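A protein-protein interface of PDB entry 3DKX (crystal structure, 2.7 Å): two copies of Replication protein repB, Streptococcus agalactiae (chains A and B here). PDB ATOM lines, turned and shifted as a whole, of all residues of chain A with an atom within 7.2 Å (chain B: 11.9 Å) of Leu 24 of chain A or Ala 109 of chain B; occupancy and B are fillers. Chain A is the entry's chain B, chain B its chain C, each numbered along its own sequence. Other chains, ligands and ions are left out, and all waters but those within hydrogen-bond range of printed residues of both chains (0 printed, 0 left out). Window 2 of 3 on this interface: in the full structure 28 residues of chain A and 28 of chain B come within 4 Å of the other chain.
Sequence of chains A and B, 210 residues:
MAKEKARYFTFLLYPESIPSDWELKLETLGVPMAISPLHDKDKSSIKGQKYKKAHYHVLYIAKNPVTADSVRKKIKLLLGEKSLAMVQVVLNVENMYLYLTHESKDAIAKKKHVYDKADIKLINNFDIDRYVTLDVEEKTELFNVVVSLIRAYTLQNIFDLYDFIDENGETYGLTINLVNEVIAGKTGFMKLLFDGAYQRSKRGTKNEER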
ATOM      1  N   SER A  20      24.437  22.849  -4.639  1.00  0.00           N
ATOM      2  CA  SER A  20      23.960  23.558  -3.469  1.00  0.00           C
ATOM      3  C   SER A  20      23.236  22.614  -2.531  1.00  0.00           C
ATOM      4  O   SER A  20      23.370  22.726  -1.322  1.00  0.00           O
ATOM      5  CB  SER A  20      23.050  24.708  -3.876  1.00  0.00           C
ATOM      6  OG  SER A  20      22.035  24.241  -4.740  1.00  0.00           O
ATOM      7  N   ASP A  21      22.482  21.673  -3.093  1.00  0.00           N
ATOM      8  CA  ASP A  21      21.713  20.706  -2.296  1.00  0.00           C
ATOM      9  C   ASP A  21      22.465  19.391  -2.061  1.00  0.00           C
ATOM     10  O   ASP A  21      21.856  18.329  -1.956  1.00  0.00           O
ATOM     11  CB  ASP A  21      20.353  20.426  -2.940  1.00  0.00           C
ATOM     12  CG  ASP A  21      20.474  19.873  -4.356  1.00  0.00           C
ATOM     13  OD1 ASP A  21      21.613  19.705  -4.845  1.00  0.00           O
ATOM     14  OD2 ASP A  21      19.429  19.614  -4.983  1.00  0.00           O
ATOM     15  N   TRP A  22      23.790  19.478  -1.969  1.00  0.00           N
ATOM     16  CA  TRP A  22      24.641  18.332  -1.681  1.00  0.00           C
ATOM     17  C   TRP A  22      24.167  17.548  -0.463  1.00  0.00           C
ATOM     18  O   TRP A  22      24.315  16.345  -0.426  1.00  0.00           O
ATOM     19  CB  TRP A  22      26.072  18.806  -1.420  1.00  0.00           C
ATOM     20  CG  TRP A  22      26.148  19.789  -0.288  1.00  0.00           C
ATOM     21  CD1 TRP A  22      25.937  21.129  -0.364  1.00  0.00           C
ATOM     22  CD2 TRP A  22      26.446  19.509   1.090  1.00  0.00           C
ATOM     23  NE1 TRP A  22      26.091  21.706   0.868  1.00  0.00           N
ATOM     24  CE2 TRP A  22      26.404  20.737   1.781  1.00  0.00           C
ATOM     25  CE3 TRP A  22      26.752  18.341   1.805  1.00  0.00           C
ATOM     26  CZ2 TRP A  22      26.647  20.837   3.154  1.00  0.00           C
ATOM     27  CZ3 TRP A  22      26.998  18.441   3.170  1.00  0.00           C
ATOM     28  CH2 TRP A  22      26.940  19.683   3.830  1.00  0.00           C
ATOM     29  N   GLU A  23      23.641  18.237   0.545  1.00  0.00           N
ATOM     30  CA  GLU A  23      23.251  17.595   1.790  1.00  0.00           C
ATOM     31  C   GLU A  23      22.103  16.614   1.575  1.00  0.00           C
ATOM     32  O   GLU A  23      22.178  15.456   1.988  1.00  0.00           O
ATOM     33  CB  GLU A  23      22.902  18.630   2.859  1.00  0.00           C
ATOM     34  CG  GLU A  23      21.914  18.121   3.891  1.00  0.00           C
ATOM     35  CD  GLU A  23      21.976  18.850   5.233  1.00  0.00           C
ATOM     36  OE1 GLU A  23      22.175  20.075   5.259  1.00  0.00           O
ATOM     37  OE2 GLU A  23      21.812  18.184   6.276  1.00  0.00           O
ATOM     38  N   LEU A  24      21.046  17.073   0.912  1.00  0.00           N
ATOM     39  CA  LEU A  24      19.923  16.209   0.542  1.00  0.00           C
ATOM     40  C   LEU A  24      20.332  15.060  -0.381  1.00  0.00           C
ATOM     41  O   LEU A  24      19.727  14.002  -0.351  1.00  0.00           O
ATOM     42  CB  LEU A  24      18.834  17.046  -0.121  1.00  0.00           C
ATOM     43  CG  LEU A  24      17.721  16.344  -0.887  1.00  0.00           C
ATOM     44  CD1 LEU A  24      16.560  16.003   0.050  1.00  0.00           C
ATOM     45  CD2 LEU A  24      17.249  17.238  -2.032  1.00  0.00           C
ATOM     46  N   LYS A  25      21.351  15.268  -1.204  1.00  0.00           N
ATOM     47  CA  LYS A  25      21.837  14.231  -2.101  1.00  0.00           C
ATOM     48  C   LYS A  25      22.564  13.129  -1.348  1.00  0.00           C
ATOM     49  O   LYS A  25      22.317  11.954  -1.569  1.00  0.00           O
ATOM     50  CB  LYS A  25      22.764  14.818  -3.152  1.00  0.00           C
ATOM     51  CG  LYS A  25      22.075  15.634  -4.208  1.00  0.00           C
ATOM     52  CD  LYS A  25      23.041  15.973  -5.348  1.00  0.00           C
ATOM     53  CE  LYS A  25      22.398  16.836  -6.425  1.00  0.00           C
ATOM     54  NZ  LYS A  25      21.397  16.039  -7.146  1.00  0.00           N
ATOM     55  N   LEU A  26      23.475  13.508  -0.466  1.00  0.00           N
ATOM     56  CA  LEU A  26      24.169  12.542   0.369  1.00  0.00           C
ATOM     57  C   LEU A  26      23.151  11.683   1.112  1.00  0.00           C
ATOM     58  O   LEU A  26      23.410  10.526   1.429  1.00  0.00           O
ATOM     59  CB  LEU A  26      25.062  13.260   1.379  1.00  0.00           C
ATOM     60  CG  LEU A  26      26.361  13.946   0.943  1.00  0.00           C
ATOM     61  CD1 LEU A  26      26.959  14.668   2.134  1.00  0.00           C
ATOM     62  CD2 LEU A  26      27.377  12.970   0.339  1.00  0.00           C
ATOM     63  N   GLU A  27      21.988  12.268   1.388  1.00  0.00           N
ATOM     64  CA  GLU A  27      20.917  11.586   2.096  1.00  0.00           C
ATOM     65  C   GLU A  27      20.322  10.459   1.255  1.00  0.00           C
ATOM     66  O   GLU A  27      19.816   9.486   1.787  1.00  0.00           O
ATOM     67  CB  GLU A  27      19.826  12.586   2.482  1.00  0.00           C
ATOM     68  CG  GLU A  27      19.005  12.225   3.703  1.00  0.00           C
ATOM     69  CD  GLU A  27      17.734  13.051   3.805  1.00  0.00           C
ATOM     70  OE1 GLU A  27      17.110  13.070   4.893  1.00  0.00           O
ATOM     71  OE2 GLU A  27      17.349  13.691   2.793  1.00  0.00           O
ATOM     72  N   THR A  28      20.387  10.590  -0.064  1.00  0.00           N
ATOM     73  CA  THR A  28      19.727   9.628  -0.950  1.00  0.00           C
ATOM     74  C   THR A  28      20.511   8.322  -1.035  1.00  0.00           C
ATOM     75  O   THR A  28      20.039   7.345  -1.611  1.00  0.00           O
ATOM     76  CB  THR A  28      19.519  10.202  -2.367  1.00  0.00           C
ATOM     77  OG1 THR A  28      20.787  10.366  -3.005  1.00  0.00           O
ATOM     78  CG2 THR A  28      18.820  11.525  -2.301  1.00  0.00           C
ATOM     79  N   LEU A  29      21.697   8.313  -0.444  1.00  0.00           N
ATOM     80  CA  LEU A  29      22.558   7.140  -0.445  1.00  0.00           C
ATOM     81  C   LEU A  29      22.143   6.117   0.600  1.00  0.00           C
ATOM     82  O   LEU A  29      22.654   5.010   0.621  1.00  0.00           O
ATOM     83  CB  LEU A  29      24.003   7.551  -0.184  1.00  0.00           C
ATOM     84  CG  LEU A  29      24.635   8.344  -1.310  1.00  0.00           C
ATOM     85  CD1 LEU A  29      26.104   8.392  -1.107  1.00  0.00           C
ATOM     86  CD2 LEU A  29      24.323   7.679  -2.617  1.00  0.00           C
ATOM     87  N   LEU A  78      27.588  10.896  -7.299  1.00  0.00           N
ATOM     88  CA  LEU A  78      26.519  11.605  -6.624  1.00  0.00           C
ATOM     89  C   LEU A  78      26.685  13.118  -6.788  1.00  0.00           C
ATOM     90  O   LEU A  78      25.737  13.837  -7.072  1.00  0.00           O
ATOM     91  CB  LEU A  78      26.544  11.243  -5.146  1.00  0.00           C
ATOM     92  CG  LEU A  78      25.262  11.273  -4.329  1.00  0.00           C
ATOM     93  CD1 LEU A  78      25.522  11.942  -2.990  1.00  0.00           C
ATOM     94  CD2 LEU A  78      24.167  11.977  -5.070  1.00  0.00           C
ATOM     95  N   ILE A 123      23.180  12.838   9.139  1.00  0.00           N
ATOM     96  CA  ILE A 123      22.383  12.216   8.082  1.00  0.00           C
ATOM     97  C   ILE A 123      21.997  10.771   8.396  1.00  0.00           C
ATOM     98  O   ILE A 123      22.803   9.997   8.918  1.00  0.00           O
ATOM     99  CB  ILE A 123      23.125  12.183   6.727  1.00  0.00           C
ATOM    100  CG1 ILE A 123      23.840  13.505   6.452  1.00  0.00           C
ATOM    101  CG2 ILE A 123      22.143  11.833   5.601  1.00  0.00           C
ATOM    102  CD1 ILE A 123      22.900  14.653   6.230  1.00  0.00           C
ATOM    103  N   LYS B  43       4.735  18.249 -13.159  1.00  0.00           N
ATOM    104  CA  LYS B  43       4.558  19.653 -13.564  1.00  0.00           C
ATOM    105  C   LYS B  43       5.595  20.149 -14.569  1.00  0.00           C
ATOM    106  O   LYS B  43       6.795  19.968 -14.386  1.00  0.00           O
ATOM    107  CB  LYS B  43       4.500  20.576 -12.354  1.00  0.00           C
ATOM    108  CG  LYS B  43       3.078  20.753 -11.813  1.00  0.00           C
ATOM    109  CD  LYS B  43       3.103  21.032 -10.311  1.00  0.00           C
ATOM    110  CE  LYS B  43       1.704  21.239  -9.732  1.00  0.00           C
ATOM    111  NZ  LYS B  43       1.741  21.069  -8.235  1.00  0.00           N
ATOM    112  N   LEU B  91      22.304   4.309  -6.939  1.00  0.00           N
ATOM    113  CA  LEU B  91      23.165   4.074  -5.808  1.00  0.00           C
ATOM    114  C   LEU B  91      22.391   3.584  -4.598  1.00  0.00           C
ATOM    115  O   LEU B  91      22.949   2.908  -3.750  1.00  0.00           O
ATOM    116  CB  LEU B  91      23.984   5.324  -5.487  1.00  0.00           C
ATOM    117  CG  LEU B  91      24.677   5.902  -6.720  1.00  0.00           C
ATOM    118  CD1 LEU B  91      25.304   7.252  -6.427  1.00  0.00           C
ATOM    119  CD2 LEU B  91      25.718   4.921  -7.227  1.00  0.00           C
ATOM    120  N   ASN B  92      21.118   3.926  -4.495  1.00  0.00           N
ATOM    121  CA  ASN B  92      20.320   3.388  -3.407  1.00  0.00           C
ATOM    122  C   ASN B  92      18.947   2.869  -3.870  1.00  0.00           C
ATOM    123  O   ASN B  92      17.987   3.638  -4.011  1.00  0.00           O
ATOM    124  CB  ASN B  92      20.171   4.415  -2.304  1.00  0.00           C
ATOM    125  CG  ASN B  92      19.227   3.956  -1.237  1.00  0.00           C
ATOM    126  OD1 ASN B  92      18.806   2.814  -1.256  1.00  0.00           O
ATOM    127  ND2 ASN B  92      18.871   4.834  -0.312  1.00  0.00           N
ATOM    128  N   ASN B  95      15.879   4.101  -2.347  1.00  0.00           N
ATOM    129  CA  ASN B  95      15.561   5.487  -2.658  1.00  0.00           C
ATOM    130  C   ASN B  95      14.852   5.582  -4.008  1.00  0.00           C
ATOM    131  O   ASN B  95      13.784   6.204  -4.131  1.00  0.00           O
ATOM    132  CB  ASN B  95      16.798   6.375  -2.623  1.00  0.00           C
ATOM    133  CG  ASN B  95      16.455   7.839  -2.774  1.00  0.00           C
ATOM    134  OD1 ASN B  95      15.933   8.472  -1.851  1.00  0.00           O
ATOM    135  ND2 ASN B  95      16.731   8.384  -3.949  1.00  0.00           N
ATOM    136  N   MET B  96      15.425   4.929  -5.015  1.00  0.00           N
ATOM    137  CA  MET B  96      14.837   5.004  -6.336  1.00  0.00           C
ATOM    138  C   MET B  96      13.437   4.365  -6.370  1.00  0.00           C
ATOM    139  O   MET B  96      12.535   4.866  -7.049  1.00  0.00           O
ATOM    140  CB  MET B  96      15.759   4.399  -7.387  1.00  0.00           C
ATOM    141  CG  MET B  96      15.113   4.325  -8.755  1.00  0.00           C
ATOM    142  SD  MET B  96      14.726   5.952  -9.518  1.00  0.00           S
ATOM    143  CE  MET B  96      16.344   6.316 -10.212  1.00  0.00           C
ATOM    144  N   LEU B  98      11.269   4.221  -3.995  1.00  0.00           N
ATOM    145  CA  LEU B  98      10.331   5.165  -3.400  1.00  0.00           C
ATOM    146  C   LEU B  98      10.132   6.361  -4.321  1.00  0.00           C
ATOM    147  O   LEU B  98       9.139   7.071  -4.240  1.00  0.00           O
ATOM    148  CB  LEU B  98      10.825   5.628  -2.033  1.00  0.00           C
ATOM    149  CG  LEU B  98      10.608   4.609  -0.910  1.00  0.00           C
ATOM    150  CD1 LEU B  98      11.474   4.928   0.303  1.00  0.00           C
ATOM    151  CD2 LEU B  98       9.135   4.557  -0.535  1.00  0.00           C
ATOM    152  N   TYR B  99      11.078   6.580  -5.217  1.00  0.00           N
ATOM    153  CA  TYR B  99      10.961   7.715  -6.100  1.00  0.00           C
ATOM    154  C   TYR B  99       9.940   7.459  -7.212  1.00  0.00           C
ATOM    155  O   TYR B  99       9.463   8.401  -7.844  1.00  0.00           O
ATOM    156  CB  TYR B  99      12.330   8.044  -6.682  1.00  0.00           C
ATOM    157  CG  TYR B  99      12.367   9.266  -7.544  1.00  0.00           C
ATOM    158  CD1 TYR B  99      12.298   9.168  -8.925  1.00  0.00           C
ATOM    159  CD2 TYR B  99      12.484  10.525  -6.978  1.00  0.00           C
ATOM    160  CE1 TYR B  99      12.337  10.302  -9.721  1.00  0.00           C
ATOM    161  CE2 TYR B  99      12.525  11.665  -7.766  1.00  0.00           C
ATOM    162  CZ  TYR B  99      12.457  11.549  -9.134  1.00  0.00           C
ATOM    163  OH  TYR B  99      12.513  12.697  -9.904  1.00  0.00           O
ATOM    164  N   THR B 101       7.038   6.769  -7.023  1.00  0.00           N
ATOM    165  CA  THR B 101       5.763   7.372  -6.653  1.00  0.00           C
ATOM    166  C   THR B 101       6.053   8.679  -5.958  1.00  0.00           C
ATOM    167  O   THR B 101       5.186   9.261  -5.301  1.00  0.00           O
ATOM    168  CB  THR B 101       4.901   6.445  -5.719  1.00  0.00           C
ATOM    169  OG1 THR B 101       5.510   6.314  -4.426  1.00  0.00           O
ATOM    170  CG2 THR B 101       4.732   5.070  -6.340  1.00  0.00           C
ATOM    171  N   HIS B 102       7.295   9.130  -6.102  1.00  0.00           N
ATOM    172  CA  HIS B 102       7.707  10.407  -5.550  1.00  0.00           C
ATOM    173  C   HIS B 102       7.517  10.434  -4.033  1.00  0.00           C
ATOM    174  O   HIS B 102       6.998  11.397  -3.492  1.00  0.00           O
ATOM    175  CB  HIS B 102       6.915  11.544  -6.199  1.00  0.00           C
ATOM    176  CG  HIS B 102       7.369  11.889  -7.590  1.00  0.00           C
ATOM    177  ND1 HIS B 102       6.555  12.529  -8.505  1.00  0.00           N
ATOM    178  CD2 HIS B 102       8.554  11.691  -8.217  1.00  0.00           C
ATOM    179  CE1 HIS B 102       7.217  12.696  -9.636  1.00  0.00           C
ATOM    180  NE2 HIS B 102       8.434  12.203  -9.486  1.00  0.00           N
ATOM    181  N   GLU B 103       7.937   9.373  -3.355  1.00  0.00           N
ATOM    182  CA  GLU B 103       7.811   9.295  -1.903  1.00  0.00           C
ATOM    183  C   GLU B 103       9.171   9.126  -1.215  1.00  0.00           C
ATOM    184  O   GLU B 103       9.227   8.833  -0.029  1.00  0.00           O
ATOM    185  CB  GLU B 103       6.869   8.154  -1.485  1.00  0.00           C
ATOM    186  CG  GLU B 103       5.591   8.088  -2.284  1.00  0.00           C
ATOM    187  CD  GLU B 103       4.394   7.601  -1.478  1.00  0.00           C
ATOM    188  OE1 GLU B 103       3.656   6.707  -1.974  1.00  0.00           O
ATOM    189  OE2 GLU B 103       4.189   8.121  -0.356  1.00  0.00           O
ATOM    190  N   SER B 104      10.258   9.291  -1.964  1.00  0.00           N
ATOM    191  CA  SER B 104      11.580   9.436  -1.374  1.00  0.00           C
ATOM    192  C   SER B 104      11.714  10.814  -0.705  1.00  0.00           C
ATOM    193  O   SER B 104      10.985  11.750  -1.040  1.00  0.00           O
ATOM    194  CB  SER B 104      12.650   9.252  -2.443  1.00  0.00           C
ATOM    195  OG  SER B 104      12.356  10.039  -3.591  1.00  0.00           O
ATOM    196  N   LYS B 105      12.632  10.933   0.254  1.00  0.00           N
ATOM    197  CA  LYS B 105      12.879  12.221   0.950  1.00  0.00           C
ATOM    198  C   LYS B 105      13.144  13.347  -0.048  1.00  0.00           C
ATOM    199  O   LYS B 105      12.529  14.407   0.039  1.00  0.00           O
ATOM    200  CB  LYS B 105      14.059  12.113   1.920  1.00  0.00           C
ATOM    201  CG  LYS B 105      13.833  11.205   3.121  1.00  0.00           C
ATOM    202  CD  LYS B 105      15.154  10.588   3.609  1.00  0.00           C
ATOM    203  CE  LYS B 105      15.199  10.476   5.134  1.00  0.00           C
ATOM    204  NZ  LYS B 105      14.586   9.216   5.646  1.00  0.00           N
ATOM    205  N   ASP B 106      14.047  13.094  -0.998  1.00  0.00           N
ATOM    206  CA  ASP B 106      14.403  14.073  -2.009  1.00  0.00           C
ATOM    207  C   ASP B 106      13.199  14.548  -2.845  1.00  0.00           C
ATOM    208  O   ASP B 106      13.056  15.740  -3.106  1.00  0.00           O
ATOM    209  CB  ASP B 106      15.555  13.575  -2.902  1.00  0.00           C
ATOM    210  CG  ASP B 106      15.251  12.249  -3.575  1.00  0.00           C
ATOM    211  OD1 ASP B 106      14.996  11.256  -2.859  1.00  0.00           O
ATOM    212  OD2 ASP B 106      15.276  12.181  -4.822  1.00  0.00           O
ATOM    213  N   ALA B 107      12.333  13.630  -3.262  1.00  0.00           N
ATOM    214  CA  ALA B 107      11.196  14.023  -4.096  1.00  0.00           C
ATOM    215  C   ALA B 107      10.185  14.778  -3.248  1.00  0.00           C
ATOM    216  O   ALA B 107       9.576  15.745  -3.710  1.00  0.00           O
ATOM    217  CB  ALA B 107      10.546  12.802  -4.762  1.00  0.00           C
ATOM    218  N   ILE B 108      10.006  14.331  -2.005  1.00  0.00           N
ATOM    219  CA  ILE B 108       9.147  15.054  -1.078  1.00  0.00           C
ATOM    220  C   ILE B 108       9.727  16.441  -0.902  1.00  0.00           C
ATOM    221  O   ILE B 108       9.015  17.452  -0.931  1.00  0.00           O
ATOM    222  CB  ILE B 108       9.077  14.371   0.291  1.00  0.00           C
ATOM    223  CG1 ILE B 108       8.064  13.224   0.256  1.00  0.00           C
ATOM    224  CG2 ILE B 108       8.667  15.371   1.360  1.00  0.00           C
ATOM    225  CD1 ILE B 108       8.322  12.132   1.277  1.00  0.00           C
ATOM    226  N   ALA B 109      11.044  16.462  -0.730  1.00  0.00           N
ATOM    227  CA  ALA B 109      11.807  17.681  -0.589  1.00  0.00           C
ATOM    228  C   ALA B 109      11.492  18.658  -1.720  1.00  0.00           C
ATOM    229  O   ALA B 109      11.083  19.791  -1.469  1.00  0.00           O
ATOM    230  CB  ALA B 109      13.290  17.343  -0.573  1.00  0.00           C
ATOM    231  N   LYS B 110      11.701  18.221  -2.959  1.00  0.00           N
ATOM    232  CA  LYS B 110      11.399  19.035  -4.129  1.00  0.00           C
ATOM    233  C   LYS B 110       9.894  19.162  -4.358  1.00  0.00           C
ATOM    234  O   LYS B 110       9.452  19.589  -5.432  1.00  0.00           O
ATOM    235  CB  LYS B 110      12.074  18.449  -5.357  1.00  0.00           C
ATOM    236  CG  LYS B 110      13.556  18.265  -5.175  1.00  0.00           C
ATOM    237  CD  LYS B 110      14.199  17.767  -6.460  1.00  0.00           C
ATOM    238  CE  LYS B 110      15.703  17.598  -6.280  1.00  0.00           C
ATOM    239  NZ  LYS B 110      16.452  17.727  -7.573  1.00  0.00           N
ATOM    240  N   LYS B 111       9.132  18.781  -3.333  1.00  0.00           N
ATOM    241  CA  LYS B 111       7.661  18.764  -3.335  1.00  0.00           C
ATOM    242  C   LYS B 111       7.022  18.293  -4.646  1.00  0.00           C
ATOM    243  O   LYS B 111       6.134  18.948  -5.168  1.00  0.00           O
ATOM    244  CB  LYS B 111       7.124  20.136  -2.946  1.00  0.00           C
ATOM    245  CG  LYS B 111       7.650  21.226  -3.852  1.00  0.00           C
ATOM    246  CD  LYS B 111       7.430  22.652  -3.293  1.00  0.00           C
ATOM    247  CE  LYS B 111       7.770  23.704  -4.376  1.00  0.00           C
ATOM    248  NZ  LYS B 111       6.846  24.881  -4.333  1.00  0.00           N
ATOM    249  N   LYS B 112       7.455  17.148  -5.161  1.00  0.00           N
ATOM    250  CA  LYS B 112       6.885  16.603  -6.384  1.00  0.00           C
ATOM    251  C   LYS B 112       5.544  15.932  -6.132  1.00  0.00           C
ATOM    252  O   LYS B 112       5.117  15.787  -4.994  1.00  0.00           O
ATOM    253  CB  LYS B 112       7.855  15.623  -7.033  1.00  0.00           C
ATOM    254  CG  LYS B 112       9.273  16.161  -7.086  1.00  0.00           C
ATOM    255  CD  LYS B 112      10.158  15.388  -8.015  1.00  0.00           C
ATOM    256  CE  LYS B 112       9.904  15.784  -9.424  1.00  0.00           C
ATOM    257  NZ  LYS B 112      11.196  15.761 -10.172  1.00  0.00           N
ATOM    258  N   HIS B 113       4.882  15.520  -7.204  1.00  0.00           N
ATOM    259  CA  HIS B 113       3.509  15.023  -7.133  1.00  0.00           C
ATOM    260  C   HIS B 113       3.491  13.555  -6.738  1.00  0.00           C
ATOM    261  O   HIS B 113       4.232  12.743  -7.308  1.00  0.00           O
ATOM    262  CB  HIS B 113       2.828  15.208  -8.488  1.00  0.00           C
ATOM    263  CG  HIS B 113       1.461  14.602  -8.572  1.00  0.00           C
ATOM    264  ND1 HIS B 113       1.255  13.252  -8.792  1.00  0.00           N
ATOM    265  CD2 HIS B 113       0.230  15.164  -8.489  1.00  0.00           C
ATOM    266  CE1 HIS B 113      -0.045  13.011  -8.828  1.00  0.00           C
ATOM    267  NE2 HIS B 113      -0.689  14.153  -8.648  1.00  0.00           N
ATOM    268  N   VAL B 114       2.644  13.222  -5.767  1.00  0.00           N
ATOM    269  CA  VAL B 114       2.564  11.847  -5.265  1.00  0.00           C
ATOM    270  C   VAL B 114       1.663  10.934  -6.087  1.00  0.00           C
ATOM    271  O   VAL B 114       0.506  11.257  -6.363  1.00  0.00           O
ATOM    272  CB  VAL B 114       2.075  11.799  -3.820  1.00  0.00           C
ATOM    273  CG1 VAL B 114       2.227  10.396  -3.282  1.00  0.00           C
ATOM    274  CG2 VAL B 114       2.843  12.806  -2.971  1.00  0.00           C
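No position is printed for both chains.
O of Thr 28 of chain A sits close to ND2 of Asn 92 of chain B.
Asp 106 of chain B touches Leu 24 of chain A (CA to CD1, 3.6 Å). CD1 of Leu 24 of chain A touches CB of Ala 109 of chain B (3.6 Å). Glu 27 of chain A touches Lys 105 of chain B. Asn 95 of chain B touches Thr 28 of chain A. CG2 of Thr 28 of chain A touches CG of Asp 106 of chain B, at 3.9 Å. CB of Leu 91 of chain B touches CD2 of Leu 29 of chain A, at 3.7 Å. ND2 of Asn 92 of chain B touches C of Leu 29 of chain A (3.6 Å).
No residue of chain B comes within 4 Å of Trp 22 of chain A. Of the printed residues of chain B, Leu 24 of chain A touches Asp 106 and Ala 109. Of chain B, only Lys 105 (3.2 Å) comes within 4 Å of Glu 27 of chain A. Of the printed residues of chain B, Thr 28 of chain A touches Asn 92 (3.0 Å), Asn 95 (3.5 Å) and Asp 106 (3.9 Å). Of the printed residues of chain A, Asn 92 of chain B touches Thr 28 (3.0 Å) and Leu 29 (3.6 Å). Thr 101 of chain B touches none of the printed residues of chain A. Printed residues of chain A within 4 Å of Lys 105 of chain B: Glu 27. Of the printed residues of chain A, Asp 106 of chain B touches Leu 24 and Thr 28. The nearest residue of chain B that does not touch Leu 24 of chain A is Lys 105 of chain B (4.3 Å). The nearest residue of chain A that does not touch Ala 109 of chain B is Glu 27 of chain A (6.4 Å). The nearest printed residue of chain A that does not touch Lys 105 of chain B is Leu 24 of chain A (4.3 Å).
Printed residues of chain B that touch a printed residue of chain A: Leu 91, Asn 92, Asn 95, Lys 105, Asp 106 and Ala 109. Along chain B the printed residues that touch a printed residue of chain A span positions 91 to 109. Among the printed residues, no Asp or Glu carboxylate lies within 4 Å of a Lys or Arg side-chain nitrogen of the other chain.
OD1 of Asn 92 of chain B is in hydrogen-bond range of N of Asn 95 of chain B, at 3.4 Å. OG1 of Thr 28 of chain A sits at hydrogen-bond distance from O of Lys 25 of chain A (2.6 Å). OD1 of Asp 106 of chain B sits close to OD1 of Asn 95 of chain B, at 3.1 Å. The side-chain carboxylate (OD1) of Asp 106 of chain B is in hydrogen-bond range of the side-chain hydroxyl (OG) of Ser 104 of chain B.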
